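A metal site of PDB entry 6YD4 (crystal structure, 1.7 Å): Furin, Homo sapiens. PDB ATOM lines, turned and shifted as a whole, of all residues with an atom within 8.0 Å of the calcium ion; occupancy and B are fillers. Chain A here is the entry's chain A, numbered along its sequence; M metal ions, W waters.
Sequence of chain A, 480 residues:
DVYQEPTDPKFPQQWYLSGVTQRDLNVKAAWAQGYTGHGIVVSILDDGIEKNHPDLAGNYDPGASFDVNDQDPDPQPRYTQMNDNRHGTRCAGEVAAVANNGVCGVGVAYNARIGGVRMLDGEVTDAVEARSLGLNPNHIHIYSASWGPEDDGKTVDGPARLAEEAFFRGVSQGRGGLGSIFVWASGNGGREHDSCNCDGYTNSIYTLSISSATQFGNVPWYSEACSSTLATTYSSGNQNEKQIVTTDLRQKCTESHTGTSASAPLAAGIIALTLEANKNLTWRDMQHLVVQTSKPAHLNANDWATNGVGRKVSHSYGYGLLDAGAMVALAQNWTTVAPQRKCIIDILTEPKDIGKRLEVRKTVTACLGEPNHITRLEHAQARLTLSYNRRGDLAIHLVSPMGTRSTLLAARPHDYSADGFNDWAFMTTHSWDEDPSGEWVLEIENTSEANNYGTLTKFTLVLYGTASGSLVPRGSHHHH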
ATOM      1  N   LYS A  51       6.145  29.497   5.076  1.00  0.00           N
ATOM      2  CA  LYS A  51       5.742  30.728   5.747  1.00  0.00           C
ATOM      3  C   LYS A  51       6.362  30.876   7.124  1.00  0.00           C
ATOM      4  O   LYS A  51       6.441  32.005   7.629  1.00  0.00           O
ATOM      5  CB  LYS A  51       4.217  30.816   5.825  1.00  0.00           C
ATOM      6  CG  LYS A  51       3.546  29.747   6.650  1.00  0.00           C
ATOM      7  CD  LYS A  51       2.024  29.773   6.462  1.00  0.00           C
ATOM      8  CE  LYS A  51       1.362  28.723   7.347  1.00  0.00           C
ATOM      9  NZ  LYS A  51       1.722  27.323   6.953  1.00  0.00           N
ATOM     10  N   PHE A  66      -2.156  31.793  -1.143  1.00  0.00           N
ATOM     11  CA  PHE A  66      -3.251  30.843  -1.313  1.00  0.00           C
ATOM     12  C   PHE A  66      -2.645  29.552  -1.837  1.00  0.00           C
ATOM     13  O   PHE A  66      -1.529  29.542  -2.364  1.00  0.00           O
ATOM     14  CB  PHE A  66      -4.333  31.376  -2.251  1.00  0.00           C
ATOM     15  CG  PHE A  66      -5.660  30.699  -2.072  1.00  0.00           C
ATOM     16  CD1 PHE A  66      -6.460  31.036  -0.999  1.00  0.00           C
ATOM     17  CD2 PHE A  66      -6.088  29.702  -2.933  1.00  0.00           C
ATOM     18  CE1 PHE A  66      -7.674  30.405  -0.792  1.00  0.00           C
ATOM     19  CE2 PHE A  66      -7.298  29.061  -2.735  1.00  0.00           C
ATOM     20  CZ  PHE A  66      -8.092  29.428  -1.660  1.00  0.00           C
ATOM     21  N   ASP A  67      -3.386  28.460  -1.659  1.00  0.00           N
ATOM     22  CA  ASP A  67      -3.005  27.147  -2.184  1.00  0.00           C
ATOM     23  C   ASP A  67      -4.037  26.754  -3.218  1.00  0.00           C
ATOM     24  O   ASP A  67      -5.113  26.242  -2.872  1.00  0.00           O
ATOM     25  CB  ASP A  67      -2.900  26.138  -1.067  1.00  0.00           C
ATOM     26  CG  ASP A  67      -2.437  24.763  -1.548  1.00  0.00           C
ATOM     27  OD1 ASP A  67      -2.417  24.511  -2.776  1.00  0.00           O
ATOM     28  OD2 ASP A  67      -2.102  23.932  -0.669  1.00  0.00           O
ATOM     29  N   VAL A  68      -3.709  26.995  -4.480  1.00  0.00           N
ATOM     30  CA  VAL A  68      -4.620  26.675  -5.567  1.00  0.00           C
ATOM     31  C   VAL A  68      -4.575  25.187  -5.868  1.00  0.00           C
ATOM     32  O   VAL A  68      -5.568  24.627  -6.330  1.00  0.00           O
ATOM     33  CB  VAL A  68      -4.265  27.509  -6.815  1.00  0.00           C
ATOM     34  CG1 VAL A  68      -5.141  27.128  -7.962  1.00  0.00           C
ATOM     35  CG2 VAL A  68      -4.415  28.997  -6.491  1.00  0.00           C
ATOM     36  N   ASN A  69      -3.439  24.524  -5.639  1.00  0.00           N
ATOM     37  CA  ASN A  69      -3.363  23.104  -5.943  1.00  0.00           C
ATOM     38  C   ASN A  69      -4.296  22.281  -5.057  1.00  0.00           C
ATOM     39  O   ASN A  69      -4.951  21.346  -5.533  1.00  0.00           O
ATOM     40  CB  ASN A  69      -1.929  22.577  -5.792  1.00  0.00           C
ATOM     41  CG  ASN A  69      -0.978  23.139  -6.826  1.00  0.00           C
ATOM     42  OD1 ASN A  69       0.111  23.614  -6.488  1.00  0.00           O
ATOM     43  ND2 ASN A  69      -1.355  23.070  -8.100  1.00  0.00           N
ATOM     44  N   ASP A  70      -4.367  22.596  -3.758  1.00  0.00           N
ATOM     45  CA  ASP A  70      -5.202  21.849  -2.817  1.00  0.00           C
ATOM     46  C   ASP A  70      -6.437  22.633  -2.383  1.00  0.00           C
ATOM     47  O   ASP A  70      -7.214  22.117  -1.569  1.00  0.00           O
ATOM     48  CB  ASP A  70      -4.393  21.453  -1.577  1.00  0.00           C
ATOM     49  CG  ASP A  70      -3.533  20.229  -1.802  1.00  0.00           C
ATOM     50  OD1 ASP A  70      -3.708  19.532  -2.824  1.00  0.00           O
ATOM     51  OD2 ASP A  70      -2.652  19.961  -0.947  1.00  0.00           O
ATOM     52  N   GLN A  71      -6.621  23.847  -2.898  1.00  0.00           N
ATOM     53  CA  GLN A  71      -7.795  24.676  -2.616  1.00  0.00           C
ATOM     54  C   GLN A  71      -7.945  24.923  -1.115  1.00  0.00           C
ATOM     55  O   GLN A  71      -8.925  24.524  -0.477  1.00  0.00           O
ATOM     56  CB  GLN A  71      -9.061  24.053  -3.247  1.00  0.00           C
ATOM     57  CG  GLN A  71      -8.985  24.070  -4.789  1.00  0.00           C
ATOM     58  CD  GLN A  71     -10.046  23.220  -5.499  1.00  0.00           C
ATOM     59  N   ASP A  72      -6.955  25.608  -0.559  1.00  0.00           N
ATOM     60  CA  ASP A  72      -6.995  26.049   0.827  1.00  0.00           C
ATOM     61  C   ASP A  72      -6.110  27.281   0.969  1.00  0.00           C
ATOM     62  O   ASP A  72      -5.400  27.659   0.016  1.00  0.00           O
ATOM     63  CB  ASP A  72      -6.564  24.936   1.801  1.00  0.00           C
ATOM     64  CG  ASP A  72      -5.091  24.565   1.710  1.00  0.00           C
ATOM     65  OD1 ASP A  72      -4.230  25.422   1.987  1.00  0.00           O
ATOM     66  OD2 ASP A  72      -4.772  23.404   1.398  1.00  0.00           O
ATOM     67  N   PRO A  73      -6.130  27.939   2.123  1.00  0.00           N
ATOM     68  CA  PRO A  73      -5.425  29.219   2.243  1.00  0.00           C
ATOM     69  C   PRO A  73      -3.944  29.092   2.498  1.00  0.00           C
ATOM     70  O   PRO A  73      -3.230  30.095   2.372  1.00  0.00           O
ATOM     71  CB  PRO A  73      -6.109  29.908   3.441  1.00  0.00           C
ATOM     72  CG  PRO A  73      -7.374  29.170   3.652  1.00  0.00           C
ATOM     73  CD  PRO A  73      -7.103  27.753   3.220  1.00  0.00           C
ATOM     74  N   ASP A  74      -3.461  27.896   2.821  1.00  0.00           N
ATOM     75  CA  ASP A  74      -2.136  27.706   3.380  1.00  0.00           C
ATOM     76  C   ASP A  74      -1.181  27.242   2.294  1.00  0.00           C
ATOM     77  O   ASP A  74      -1.277  26.081   1.859  1.00  0.00           O
ATOM     78  CB  ASP A  74      -2.206  26.683   4.512  1.00  0.00           C
ATOM     79  CG  ASP A  74      -0.874  26.401   5.155  1.00  0.00           C
ATOM     80  OD1 ASP A  74       0.148  26.975   4.735  1.00  0.00           O
ATOM     81  OD2 ASP A  74      -0.846  25.599   6.115  1.00  0.00           O
ATOM     82  N   PRO A  75      -0.221  28.098   1.863  1.00  0.00           N
ATOM     83  CA  PRO A  75       0.649  27.741   0.737  1.00  0.00           C
ATOM     84  C   PRO A  75       1.878  26.938   1.113  1.00  0.00           C
ATOM     85  O   PRO A  75       2.854  26.890   0.356  1.00  0.00           O
ATOM     86  CB  PRO A  75       1.081  29.100   0.196  1.00  0.00           C
ATOM     87  CG  PRO A  75       1.256  29.885   1.499  1.00  0.00           C
ATOM     88  CD  PRO A  75       0.073  29.462   2.361  1.00  0.00           C
ATOM     89  N   GLN A  76       1.868  26.342   2.293  1.00  0.00           N
ATOM     90  CA  GLN A  76       3.045  25.613   2.773  1.00  0.00           C
ATOM     91  C   GLN A  76       3.443  24.556   1.739  1.00  0.00           C
ATOM     92  O   GLN A  76       2.576  23.865   1.185  1.00  0.00           O
ATOM     93  CB  GLN A  76       2.745  24.920   4.104  1.00  0.00           C
ATOM     94  CG  GLN A  76       3.982  24.409   4.818  1.00  0.00           C
ATOM     95  CD  GLN A  76       4.761  25.509   5.509  1.00  0.00           C
ATOM     96  OE1 GLN A  76       4.226  26.583   5.776  1.00  0.00           O
ATOM     97  NE2 GLN A  76       6.031  25.239   5.827  1.00  0.00           N
ATOM     98  N   PRO A  77       4.731  24.417   1.452  1.00  0.00           N
ATOM     99  CA  PRO A  77       5.142  23.432   0.456  1.00  0.00           C
ATOM    100  C   PRO A  77       4.914  22.006   0.952  1.00  0.00           C
ATOM    101  O   PRO A  77       4.885  21.730   2.158  1.00  0.00           O
ATOM    102  CB  PRO A  77       6.644  23.703   0.247  1.00  0.00           C
ATOM    103  CG  PRO A  77       6.907  25.014   0.889  1.00  0.00           C
ATOM    104  CD  PRO A  77       5.866  25.209   1.963  1.00  0.00           C
ATOM    105  N   ARG A  78       4.755  21.111  -0.020  1.00  0.00           N
ATOM    106  CA  ARG A  78       4.708  19.670   0.227  1.00  0.00           C
ATOM    107  C   ARG A  78       6.128  19.150   0.376  1.00  0.00           C
ATOM    108  O   ARG A  78       6.952  19.281  -0.535  1.00  0.00           O
ATOM    109  CB  ARG A  78       3.977  18.991  -0.929  1.00  0.00           C
ATOM    110  CG  ARG A  78       3.883  17.461  -0.817  1.00  0.00           C
ATOM    111  CD  ARG A  78       2.969  16.910  -1.929  1.00  0.00           C
ATOM    112  NE  ARG A  78       3.552  17.190  -3.238  1.00  0.00           N
ATOM    113  CZ  ARG A  78       4.419  16.417  -3.871  1.00  0.00           C
ATOM    114  NH1 ARG A  78       4.908  16.790  -5.052  1.00  0.00           N
ATOM    115  NH2 ARG A  78       4.804  15.269  -3.328  1.00  0.00           N
ATOM    116  N   ARG A 118       0.655  28.576  -3.956  1.00  0.00           N
ATOM    117  CA  ARG A 118       1.044  27.198  -4.260  1.00  0.00           C
ATOM    118  C   ARG A 118       0.191  26.773  -5.435  1.00  0.00           C
ATOM    119  O   ARG A 118      -1.001  26.502  -5.293  1.00  0.00           O
ATOM    120  CB  ARG A 118       0.848  26.308  -3.036  1.00  0.00           C
ATOM    121  CG  ARG A 118       1.240  24.838  -3.282  1.00  0.00           C
ATOM    122  CD  ARG A 118       1.249  23.981  -1.947  1.00  0.00           C
ATOM    123  NE  ARG A 118       1.532  22.583  -2.294  1.00  0.00           N
ATOM    124  CZ  ARG A 118       0.621  21.606  -2.352  1.00  0.00           C
ATOM    125  NH1 ARG A 118       1.019  20.391  -2.732  1.00  0.00           N
ATOM    126  NH2 ARG A 118      -0.641  21.803  -2.005  1.00  0.00           N
HETATM  127 CA    CA M   1      -2.271  23.840   1.623  1.00  0.00          CA
HETATM  128  O   HOH W   1       0.019  23.348   2.013  1.00  0.00           O
HETATM  129  O   HOH W   2      -2.374  21.425   1.384  1.00  0.00           O
HETATM  130  O   HOH W   3      -2.467  23.333   3.949  1.00  0.00           O
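OD2 of Asp 67 binds the calcium ion.
Water W1 binds the calcium ion (2.4 Å).
The calcium ion is bound by water W3 (2.4 Å).
Water W2 binds the calcium ion (2.4 Å).
O of Asp 74 binds the calcium ion (2.5 Å).
OD1 of Asp 72 is bound to the calcium ion (2.5 Å).
The side-chain carboxylate (OD2) of Asp 72 binds the calcium ion, 2.5 Å away.
The calcium ion has seven donor atoms within binding distance.
Three residues have an atom within 4 Å of the calcium ion: Asp 67, Asp 72 and Asp 74.
The nearest printed residue that does not touch the calcium ion is Arg 118 (4.5 Å).
The side-chain carboxylate of Asp 67 lies within salt-bridge range of the guanidinium group of Arg 118 (3.3 Å).
The side-chain carboxylate (OD1) of Asp 67 lies within hydrogen-bond range of the backbone NH (N) of Asp 70 (2.9 Å).
OD1 of Asp 67 sits at hydrogen-bond distance from N of Asn 69 (3.0 Å).
The backbone NH (N) of Gln 76 sits at hydrogen-bond distance from the side-chain carboxylate (OD1) of Asp 74.
OD1 of Asp 74 lies within salt-bridge range of NZ of Lys 51.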
